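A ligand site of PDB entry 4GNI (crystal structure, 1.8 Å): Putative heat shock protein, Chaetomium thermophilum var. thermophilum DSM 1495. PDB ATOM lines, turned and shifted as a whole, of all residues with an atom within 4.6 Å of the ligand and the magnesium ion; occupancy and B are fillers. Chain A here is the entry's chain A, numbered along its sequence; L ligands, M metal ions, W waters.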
ATOM      1  N   GLY A  21       0.657  -9.755 -27.532  1.00  0.00           N
ATOM      2  CA  GLY A  21      -0.225 -10.369 -26.542  1.00  0.00           C
ATOM      3  C   GLY A  21       0.356 -10.535 -25.150  1.00  0.00           C
ATOM      4  O   GLY A  21       1.532 -10.286 -24.980  1.00  0.00           O
ATOM      5  N   ASN A  22      -0.450 -10.932 -24.159  1.00  0.00           N
ATOM      6  CA  ASN A  22       0.033 -11.051 -22.783  1.00  0.00           C
ATOM      7  C   ASN A  22       1.033 -12.235 -22.676  1.00  0.00           C
ATOM      8  O   ASN A  22       2.006 -12.176 -21.911  1.00  0.00           O
ATOM      9  CB  ASN A  22      -1.106 -11.235 -21.781  1.00  0.00           C
ATOM     10  CG  ASN A  22      -0.941 -10.353 -20.531  1.00  0.00           C
ATOM     11  OD1 ASN A  22      -0.419  -9.219 -20.614  1.00  0.00           O
ATOM     12  ND2 ASN A  22      -1.393 -10.850 -19.369  1.00  0.00           N
ATOM     13  N   SER A  23       0.809 -13.287 -23.477  1.00  0.00           N
ATOM     14  CA  SER A  23       1.652 -14.481 -23.494  1.00  0.00           C
ATOM     15  C   SER A  23       2.680 -14.501 -24.627  1.00  0.00           C
ATOM     16  O   SER A  23       3.891 -14.700 -24.396  1.00  0.00           O
ATOM     17  CB  SER A  23       0.786 -15.743 -23.537  1.00  0.00           C
ATOM     18  OG  SER A  23      -0.087 -15.821 -22.415  1.00  0.00           O
ATOM     19  N   ASN A  24       2.189 -14.354 -25.852  1.00  0.00           N
ATOM     20  CA  ASN A  24       3.031 -14.360 -27.048  1.00  0.00           C
ATOM     21  C   ASN A  24       2.835 -13.123 -27.908  1.00  0.00           C
ATOM     22  O   ASN A  24       1.832 -12.432 -27.795  1.00  0.00           O
ATOM     23  CB  ASN A  24       2.697 -15.587 -27.870  1.00  0.00           C
ATOM     24  CG  ASN A  24       3.013 -16.865 -27.138  1.00  0.00           C
ATOM     25  OD1 ASN A  24       4.132 -17.050 -26.691  1.00  0.00           O
ATOM     26  ND2 ASN A  24       2.018 -17.724 -26.980  1.00  0.00           N
ATOM     27  N   ARG A  80       1.632  -7.083 -21.032  1.00  0.00           N
ATOM     28  CA  ARG A  80       0.866  -6.424 -22.089  1.00  0.00           C
ATOM     29  C   ARG A  80      -0.358  -5.712 -21.520  1.00  0.00           C
ATOM     30  O   ARG A  80      -0.568  -4.539 -21.753  1.00  0.00           O
ATOM     31  CB  ARG A  80       0.437  -7.438 -23.166  1.00  0.00           C
ATOM     32  CG  ARG A  80       0.128  -6.868 -24.569  1.00  0.00           C
ATOM     33  CD  ARG A  80      -1.184  -6.112 -24.659  1.00  0.00           C
ATOM     34  NE  ARG A  80      -2.343  -6.864 -24.177  1.00  0.00           N
ATOM     35  CZ  ARG A  80      -3.166  -7.564 -24.955  1.00  0.00           C
ATOM     36  NH1 ARG A  80      -2.965  -7.627 -26.266  1.00  0.00           N
ATOM     37  NH2 ARG A  80      -4.210  -8.206 -24.426  1.00  0.00           N
ATOM     38  N   GLU A 186      -8.048  -7.250 -32.204  1.00  0.00           N
ATOM     39  CA  GLU A 186      -7.637  -8.638 -32.365  1.00  0.00           C
ATOM     40  C   GLU A 186      -8.678  -9.468 -33.138  1.00  0.00           C
ATOM     41  O   GLU A 186      -8.327 -10.229 -34.045  1.00  0.00           O
ATOM     42  CB  GLU A 186      -7.260  -9.244 -31.010  1.00  0.00           C
ATOM     43  CG  GLU A 186      -5.942  -8.666 -30.486  1.00  0.00           C
ATOM     44  CD  GLU A 186      -5.741  -8.862 -28.997  1.00  0.00           C
ATOM     45  OE1 GLU A 186      -6.739  -9.063 -28.283  1.00  0.00           O
ATOM     46  OE2 GLU A 186      -4.574  -8.799 -28.543  1.00  0.00           O
ATOM     47  N   ASP A 211     -11.545 -16.271 -29.560  1.00  0.00           N
ATOM     48  CA  ASP A 211     -10.114 -16.070 -29.375  1.00  0.00           C
ATOM     49  C   ASP A 211      -9.742 -16.583 -27.979  1.00  0.00           C
ATOM     50  O   ASP A 211      -9.991 -15.938 -26.965  1.00  0.00           O
ATOM     51  CB  ASP A 211      -9.749 -14.583 -29.549  1.00  0.00           C
ATOM     52  CG  ASP A 211      -8.250 -14.336 -29.611  1.00  0.00           C
ATOM     53  OD1 ASP A 211      -7.465 -15.196 -29.128  1.00  0.00           O
ATOM     54  OD2 ASP A 211      -7.858 -13.269 -30.126  1.00  0.00           O
ATOM     55  N   LEU A 212      -9.199 -17.790 -27.946  1.00  0.00           N
ATOM     56  CA  LEU A 212      -8.877 -18.437 -26.681  1.00  0.00           C
ATOM     57  C   LEU A 212      -7.366 -18.367 -26.517  1.00  0.00           C
ATOM     58  O   LEU A 212      -6.616 -18.945 -27.308  1.00  0.00           O
ATOM     59  CB  LEU A 212      -9.378 -19.882 -26.722  1.00  0.00           C
ATOM     60  CG  LEU A 212     -10.765 -20.035 -27.374  1.00  0.00           C
ATOM     61  CD1 LEU A 212     -11.192 -21.498 -27.359  1.00  0.00           C
ATOM     62  CD2 LEU A 212     -11.797 -19.161 -26.674  1.00  0.00           C
ATOM     63  N   GLY A 213      -6.924 -17.638 -25.498  1.00  0.00           N
ATOM     64  CA  GLY A 213      -5.513 -17.319 -25.367  1.00  0.00           C
ATOM     65  C   GLY A 213      -4.904 -17.960 -24.133  1.00  0.00           C
ATOM     66  O   GLY A 213      -5.273 -19.085 -23.768  1.00  0.00           O
ATOM     67  N   GLY A 214      -3.965 -17.254 -23.506  1.00  0.00           N
ATOM     68  CA  GLY A 214      -3.187 -17.841 -22.420  1.00  0.00           C
ATOM     69  C   GLY A 214      -3.678 -17.376 -21.068  1.00  0.00           C
ATOM     70  O   GLY A 214      -4.107 -18.175 -20.232  1.00  0.00           O
ATOM     71  N   SER A 215      -3.630 -16.063 -20.852  1.00  0.00           N
ATOM     72  CA  SER A 215      -4.175 -15.474 -19.638  1.00  0.00           C
ATOM     73  C   SER A 215      -5.596 -14.959 -19.839  1.00  0.00           C
ATOM     74  O   SER A 215      -6.183 -14.410 -18.914  1.00  0.00           O
ATOM     75  CB  SER A 215      -3.269 -14.333 -19.164  1.00  0.00           C
ATOM     76  OG  SER A 215      -3.246 -13.298 -20.141  1.00  0.00           O
ATOM     77  N   ARG A 216      -6.152 -15.123 -21.031  1.00  0.00           N
ATOM     78  CA  ARG A 216      -7.505 -14.651 -21.268  1.00  0.00           C
ATOM     79  C   ARG A 216      -8.150 -15.262 -22.496  1.00  0.00           C
ATOM     80  O   ARG A 216      -7.476 -15.700 -23.434  1.00  0.00           O
ATOM     81  CB  ARG A 216      -7.532 -13.126 -21.396  1.00  0.00           C
ATOM     82  CG  ARG A 216      -6.711 -12.587 -22.566  1.00  0.00           C
ATOM     83  CD  ARG A 216      -6.652 -11.052 -22.578  1.00  0.00           C
ATOM     84  NE  ARG A 216      -7.932 -10.426 -22.937  1.00  0.00           N
ATOM     85  CZ  ARG A 216      -8.157  -9.117 -22.846  1.00  0.00           C
ATOM     86  NH1 ARG A 216      -7.211  -8.307 -22.379  1.00  0.00           N
ATOM     87  NH2 ARG A 216      -9.330  -8.616 -23.211  1.00  0.00           N
ATOM     88  N   GLY A 242      -5.704 -20.931 -21.618  1.00  0.00           N
ATOM     89  CA  GLY A 242      -4.648 -21.924 -21.678  1.00  0.00           C
ATOM     90  C   GLY A 242      -3.907 -22.132 -20.361  1.00  0.00           C
ATOM     91  O   GLY A 242      -3.396 -23.237 -20.085  1.00  0.00           O
ATOM     92  N   ILE A 243      -3.821 -21.092 -19.541  1.00  0.00           N
ATOM     93  CA  ILE A 243      -3.186 -21.230 -18.226  1.00  0.00           C
ATOM     94  C   ILE A 243      -4.011 -22.154 -17.329  1.00  0.00           C
ATOM     95  O   ILE A 243      -3.449 -22.963 -16.588  1.00  0.00           O
ATOM     96  CB  ILE A 243      -2.907 -19.844 -17.562  1.00  0.00           C
ATOM     97  CG1 ILE A 243      -1.813 -19.116 -18.342  1.00  0.00           C
ATOM     98  CG2 ILE A 243      -2.493 -20.015 -16.118  1.00  0.00           C
ATOM     99  CD1 ILE A 243      -1.401 -17.780 -17.769  1.00  0.00           C
ATOM    100  N   ASP A 246      -3.059 -25.591 -18.588  1.00  0.00           N
ATOM    101  CA  ASP A 246      -1.764 -25.901 -17.991  1.00  0.00           C
ATOM    102  C   ASP A 246      -1.936 -26.430 -16.566  1.00  0.00           C
ATOM    103  O   ASP A 246      -1.335 -27.448 -16.201  1.00  0.00           O
ATOM    104  CB  ASP A 246      -0.843 -24.673 -17.978  1.00  0.00           C
ATOM    105  CG  ASP A 246      -0.392 -24.244 -19.358  1.00  0.00           C
ATOM    106  OD1 ASP A 246      -0.574 -25.016 -20.341  1.00  0.00           O
ATOM    107  OD2 ASP A 246       0.161 -23.125 -19.472  1.00  0.00           O
ATOM    108  N   GLU A 282       2.939 -27.052 -20.268  1.00  0.00           N
ATOM    109  CA  GLU A 282       2.556 -26.349 -21.488  1.00  0.00           C
ATOM    110  C   GLU A 282       3.012 -27.146 -22.698  1.00  0.00           C
ATOM    111  O   GLU A 282       2.270 -27.330 -23.648  1.00  0.00           O
ATOM    112  CB  GLU A 282       3.148 -24.948 -21.540  1.00  0.00           C
ATOM    113  CG  GLU A 282       2.814 -24.223 -22.859  1.00  0.00           C
ATOM    114  CD  GLU A 282       3.182 -22.749 -22.849  1.00  0.00           C
ATOM    115  OE1 GLU A 282       4.052 -22.365 -22.028  1.00  0.00           O
ATOM    116  OE2 GLU A 282       2.596 -21.978 -23.641  1.00  0.00           O
ATOM    117  N   LYS A 285       0.822 -30.247 -23.111  1.00  0.00           N
ATOM    118  CA  LYS A 285      -0.436 -29.725 -23.673  1.00  0.00           C
ATOM    119  C   LYS A 285      -0.379 -29.501 -25.174  1.00  0.00           C
ATOM    120  O   LYS A 285      -1.240 -29.952 -25.935  1.00  0.00           O
ATOM    121  CB  LYS A 285      -0.796 -28.409 -22.983  1.00  0.00           C
ATOM    122  CG  LYS A 285      -2.144 -27.850 -23.408  1.00  0.00           C
ATOM    123  CD  LYS A 285      -2.419 -26.510 -22.743  1.00  0.00           C
ATOM    124  CE  LYS A 285      -1.501 -25.412 -23.264  1.00  0.00           C
ATOM    125  NZ  LYS A 285      -1.800 -24.114 -22.553  1.00  0.00           N
ATOM    126  N   ARG A 286       0.633 -28.780 -25.624  1.00  0.00           N
ATOM    127  CA  ARG A 286       0.746 -28.498 -27.049  1.00  0.00           C
ATOM    128  C   ARG A 286       1.040 -29.752 -27.867  1.00  0.00           C
ATOM    129  O   ARG A 286       0.577 -29.869 -29.003  1.00  0.00           O
ATOM    130  CB  ARG A 286       1.775 -27.402 -27.274  1.00  0.00           C
ATOM    131  CG  ARG A 286       1.389 -26.127 -26.528  1.00  0.00           C
ATOM    132  CD  ARG A 286       2.510 -25.143 -26.470  1.00  0.00           C
ATOM    133  NE  ARG A 286       2.922 -24.728 -27.804  1.00  0.00           N
ATOM    134  CZ  ARG A 286       3.877 -23.843 -28.042  1.00  0.00           C
ATOM    135  NH1 ARG A 286       4.512 -23.267 -27.020  1.00  0.00           N
ATOM    136  NH2 ARG A 286       4.204 -23.520 -29.292  1.00  0.00           N
ATOM    137  N   SER A 289      -2.088 -31.568 -28.977  1.00  0.00           N
ATOM    138  CA  SER A 289      -2.887 -30.964 -30.030  1.00  0.00           C
ATOM    139  C   SER A 289      -2.491 -31.552 -31.368  1.00  0.00           C
ATOM    140  O   SER A 289      -3.251 -31.521 -32.320  1.00  0.00           O
ATOM    141  CB  SER A 289      -2.721 -29.438 -30.044  1.00  0.00           C
ATOM    142  OG  SER A 289      -3.505 -28.818 -29.040  1.00  0.00           O
ATOM    143  N   GLY A 352      -6.358 -17.705 -31.633  1.00  0.00           N
ATOM    144  CA  GLY A 352      -5.597 -17.807 -30.398  1.00  0.00           C
ATOM    145  C   GLY A 352      -4.951 -19.177 -30.279  1.00  0.00           C
ATOM    146  O   GLY A 352      -5.405 -20.130 -30.920  1.00  0.00           O
ATOM    147  N   GLY A 353      -3.910 -19.272 -29.460  1.00  0.00           N
ATOM    148  CA  GLY A 353      -3.143 -20.513 -29.381  1.00  0.00           C
ATOM    149  C   GLY A 353      -3.960 -21.686 -28.880  1.00  0.00           C
ATOM    150  O   GLY A 353      -3.771 -22.814 -29.330  1.00  0.00           O
ATOM    151  N   THR A 354      -4.880 -21.410 -27.969  1.00  0.00           N
ATOM    152  CA  THR A 354      -5.682 -22.459 -27.355  1.00  0.00           C
ATOM    153  C   THR A 354      -6.712 -23.039 -28.332  1.00  0.00           C
ATOM    154  O   THR A 354      -7.154 -24.178 -28.185  1.00  0.00           O
ATOM    155  CB  THR A 354      -6.327 -21.959 -26.041  1.00  0.00           C
ATOM    156  OG1 THR A 354      -5.284 -21.734 -25.074  1.00  0.00           O
ATOM    157  CG2 THR A 354      -7.297 -22.982 -25.489  1.00  0.00           C
ATOM    158  N   ASN A 356      -5.976 -24.138 -31.009  1.00  0.00           N
ATOM    159  CA  ASN A 356      -5.316 -25.271 -31.652  1.00  0.00           C
ATOM    160  C   ASN A 356      -5.795 -26.616 -31.127  1.00  0.00           C
ATOM    161  O   ASN A 356      -5.526 -27.658 -31.725  1.00  0.00           O
ATOM    162  CB  ASN A 356      -3.807 -25.199 -31.479  1.00  0.00           C
ATOM    163  CG  ASN A 356      -3.168 -24.197 -32.391  1.00  0.00           C
ATOM    164  OD1 ASN A 356      -3.117 -24.410 -33.611  1.00  0.00           O
ATOM    165  ND2 ASN A 356      -2.647 -23.120 -31.824  1.00  0.00           N
ATOM    166  N   THR A 357      -6.489 -26.589 -30.003  1.00  0.00           N
ATOM    167  CA  THR A 357      -6.945 -27.815 -29.351  1.00  0.00           C
ATOM    168  C   THR A 357      -8.070 -28.512 -30.135  1.00  0.00           C
ATOM    169  O   THR A 357      -9.186 -27.991 -30.214  1.00  0.00           O
ATOM    170  CB  THR A 357      -7.447 -27.543 -27.936  1.00  0.00           C
ATOM    171  OG1 THR A 357      -6.529 -26.686 -27.243  1.00  0.00           O
ATOM    172  CG2 THR A 357      -7.625 -28.841 -27.172  1.00  0.00           C
ATOM    173  N   SER A 387      -2.997 -19.640 -34.488  1.00  0.00           N
ATOM    174  CA  SER A 387      -1.997 -18.818 -33.808  1.00  0.00           C
ATOM    175  C   SER A 387      -1.432 -17.726 -34.697  1.00  0.00           C
ATOM    176  O   SER A 387      -0.756 -16.820 -34.219  1.00  0.00           O
ATOM    177  CB  SER A 387      -0.844 -19.687 -33.288  1.00  0.00           C
ATOM    178  OG  SER A 387      -1.286 -20.576 -32.276  1.00  0.00           O
ATOM    179  N   GLN A 390      -4.030 -13.429 -36.208  1.00  0.00           N
ATOM    180  CA  GLN A 390      -3.970 -12.023 -35.841  1.00  0.00           C
ATOM    181  C   GLN A 390      -2.823 -11.287 -36.534  1.00  0.00           C
ATOM    182  O   GLN A 390      -3.021 -10.197 -37.084  1.00  0.00           O
ATOM    183  CB  GLN A 390      -3.925 -11.854 -34.320  1.00  0.00           C
ATOM    184  CG  GLN A 390      -5.209 -12.311 -33.611  1.00  0.00           C
ATOM    185  CD  GLN A 390      -5.035 -12.487 -32.113  1.00  0.00           C
ATOM    186  OE1 GLN A 390      -4.958 -11.521 -31.373  1.00  0.00           O
ATOM    187  NE2 GLN A 390      -4.949 -13.754 -31.668  1.00  0.00           N
HETATM  188  P1  LIG L   1      -2.910 -13.873 -23.684  1.00  0.00           P
HETATM  189  O1  LIG L   1      -2.964 -12.445 -24.168  1.00  0.00           O
HETATM  190  O2  LIG L   1      -2.176 -14.112 -22.404  1.00  0.00           O
HETATM  191  O3  LIG L   1      -4.230 -14.610 -23.704  1.00  0.00           O
HETATM  192  P2  LIG L   1      -1.652 -14.406 -26.269  1.00  0.00           P
HETATM  193  O4  LIG L   1      -0.342 -13.692 -26.372  1.00  0.00           O
HETATM  194  O5  LIG L   1      -2.821 -13.948 -27.036  1.00  0.00           O
HETATM  195  O6  LIG L   1      -2.028 -14.690 -24.733  1.00  0.00           O
HETATM  196  P3  LIG L   1      -1.790 -16.974 -27.723  1.00  0.00           P
HETATM  197  O7  LIG L   1      -0.472 -17.342 -28.337  1.00  0.00           O
HETATM  198  O8  LIG L   1      -2.929 -16.542 -28.604  1.00  0.00           O
HETATM  199  O9  LIG L   1      -1.415 -15.977 -26.529  1.00  0.00           O
HETATM  200  O10 LIG L   1      -2.338 -18.184 -26.813  1.00  0.00           O
HETATM  201  C1  LIG L   1      -1.592 -18.613 -25.666  1.00  0.00           C
HETATM  202  C2  LIG L   1      -2.051 -19.993 -25.202  1.00  0.00           C
HETATM  203  O11 LIG L   1      -2.172 -20.877 -26.322  1.00  0.00           O
HETATM  204  C3  LIG L   1      -1.024 -20.630 -24.260  1.00  0.00           C
HETATM  205  O12 LIG L   1      -1.734 -21.121 -23.115  1.00  0.00           O
HETATM  206  C4  LIG L   1      -0.421 -21.761 -25.067  1.00  0.00           C
HETATM  207  O13 LIG L   1       0.031 -22.856 -24.257  1.00  0.00           O
HETATM  208  C5  LIG L   1      -1.589 -22.120 -25.973  1.00  0.00           C
HETATM  209  N1  LIG L   1      -1.183 -22.889 -27.171  1.00  0.00           N
HETATM  210  C6  LIG L   1      -0.283 -22.551 -28.113  1.00  0.00           C
HETATM  211  N2  LIG L   1      -0.188 -23.536 -29.047  1.00  0.00           N
HETATM  212  C7  LIG L   1      -1.041 -24.519 -28.674  1.00  0.00           C
HETATM  213  C8  LIG L   1      -1.449 -25.839 -29.186  1.00  0.00           C
HETATM  214  N3  LIG L   1      -0.896 -26.334 -30.323  1.00  0.00           N
HETATM  215  N4  LIG L   1      -2.386 -26.528 -28.490  1.00  0.00           N
HETATM  216  C9  LIG L   1      -2.943 -26.056 -27.359  1.00  0.00           C
HETATM  217  N5  LIG L   1      -2.619 -24.859 -26.840  1.00  0.00           N
HETATM  218  C10 LIG L   1      -1.685 -24.085 -27.451  1.00  0.00           C
HETATM  219 MG    MG M   1      -4.566 -12.902 -27.564  1.00  0.00          MG
HETATM  220  O   HOH W   1      -6.481 -12.051 -28.198  1.00  0.00           O
HETATM  221  O   HOH W   2      -0.786 -12.762 -29.264  1.00  0.00           O
HETATM  222  O   HOH W   3      -4.118 -11.245 -26.112  1.00  0.00           O
HETATM  223  O   HOH W   4       2.418 -20.735 -29.132  1.00  0.00           O
HETATM  224  O   HOH W   5       0.046 -21.319 -21.291  1.00  0.00           O
HETATM  225  O   HOH W   6      -2.090 -15.314 -31.191  1.00  0.00           O
HETATM  226  O   HOH W   7      -1.023 -27.637 -32.748  1.00  0.00           O
HETATM  227  O   HOH W   8      -5.624 -14.133 -25.989  1.00  0.00           O
HETATM  228  O   HOH W   9      -0.012 -19.594 -29.695  1.00  0.00           O
HETATM  229  O   HOH W  10      -4.865 -14.694 -28.924  1.00  0.00           O
HETATM  230  O   HOH W  11      -4.039 -23.956 -24.437  1.00  0.00           O
HETATM  231  O   HOH W  12      -3.478 -11.659 -29.144  1.00  0.00           O
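The backbone carbonyl oxygen (O) of Gly 214 lies within hydrogen-bond range of the backbone NH (N) of Ile 243 (3.0 Å). The backbone carbonyl oxygen of Gly 353 lies within hydrogen-bond range of the side-chain amide nitrogen of Asn 356 (2.8 Å). OD1 of Asn 22 sits at hydrogen-bond distance from N of Arg 80 (3.0 Å). The side-chain hydroxyl (OG1) of Thr 354 lies within hydrogen-bond range of the backbone carbonyl oxygen (O) of Gly 213, at 3.0 Å. The backbone carbonyl oxygen of Thr 354 sits at hydrogen-bond distance from the side-chain hydroxyl of Thr 357 (2.8 Å). The backbone carbonyl oxygen of Gly 242 is in hydrogen-bond range of the side-chain amino group of Lys 285 (3.1 Å). The backbone NH (N) of Gly 242 sits at hydrogen-bond distance from the backbone carbonyl oxygen (O) of Gly 213, 2.9 Å away. O of Gly 214 is in hydrogen-bond range of N of Gly 242, at 3.5 Å.
Water W3 lies within hydrogen-bond range of O1 of the ligand (2.6 Å), NH2 of Arg 80 (3.5 Å) and OE2 of Glu 186 (3.5 Å). Water W10 lies within hydrogen-bond range of OD1 of Asp 211, O8 of the ligand and NE2 of Gln 390. Water W9 bridges an oxygen (O7) of the ligand and the side-chain hydroxyl (OG) of Ser 387. Water W11 lies within hydrogen-bond range of OG1 of Thr 354 (2.6 Å), NZ of Lys 285 (2.9 Å) and N5 of the ligand (2.9 Å). Water W6 bridges O8 of the ligand and NE2 of Gln 390. Water W2 lies within hydrogen-bond range of O of Asn 24 (3.0 Å) and O4 of the ligand (3.1 Å).
No residue comes within 4 Å of the magnesium ion.
The side-chain carboxylate (OE2) of Glu 282 is in hydrogen-bond range of an oxygen (O13) of the ligand. The backbone NH (N) of Gly 214 is in hydrogen-bond range of an oxygen (O3) of the ligand. The backbone NH (N) of Asn 24 sits at hydrogen-bond distance from an oxygen (O4) of the ligand, at 2.7 Å. O1 of the ligand is in hydrogen-bond range of N of Asn 22, 2.9 Å away. The backbone NH (N) of Gly 353 lies within hydrogen-bond range of an oxygen (O8) of the ligand, 3.0 Å away. The side-chain amide nitrogen (ND2) of Asn 24 lies within hydrogen-bond range of an oxygen (O7) of the ligand. The side-chain amino group of Lys 285 lies within hydrogen-bond range of an oxygen (O13) of the ligand. The side-chain hydroxyl (OG) of Ser 289 is in hydrogen-bond range of a nitrogen (N4) of the ligand, 2.6 Å away. The side-chain hydroxyl (OG) of Ser 215 lies within hydrogen-bond range of an oxygen (O2) of the ligand. The backbone NH (N) of Ser 23 lies within hydrogen-bond range of an oxygen (O4) of the ligand. The backbone NH (N) of Thr 354 lies within hydrogen-bond range of an oxygen (O11) of the ligand (3.2 Å). An oxygen (O2) of the ligand lies within hydrogen-bond range of the side-chain hydroxyl of Ser 23. An oxygen (O3) of the ligand sits at hydrogen-bond distance from the backbone NH (N) of Arg 216. The backbone NH (N) of Ser 215 is in hydrogen-bond range of an oxygen (O2) of the ligand (2.9 Å). O of Asn 24 sits close to O4 of the ligand (2.9 Å). The side-chain hydroxyl of Thr 354 is in hydrogen-bond range of an oxygen (O11) of the ligand (3.5 Å).
Merely in contact with the ligand: Gly 21 (3.3 Å), Asn 356 (3.3 Å), Gly 242 (3.3 Å), Gly 213 (3.4 Å), Gly 352 (3.5 Å), Arg 286 (3.6 Å) and Thr 357 (3.6 Å). 18 residues have an atom within 4 Å of the ligand: Gly 21, Asn 22, Ser 23, Asn 24, Gly 213, Gly 214, Ser 215, Arg 216, Gly 242, Glu 282, Lys 285, Arg 286, Ser 289, Gly 352, Gly 353, Thr 354, Asn 356 and Thr 357. The nearest printed residue that does not touch the ligand is Ile 243 (4.1 Å).
The magnesium ion is bound by O5 of the ligand (2.1 Å), water W1 (2.2 Å), water W3 (2.2 Å), water W8 (2.3 Å), water W10 (2.3 Å) and water W12 (2.3 Å).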
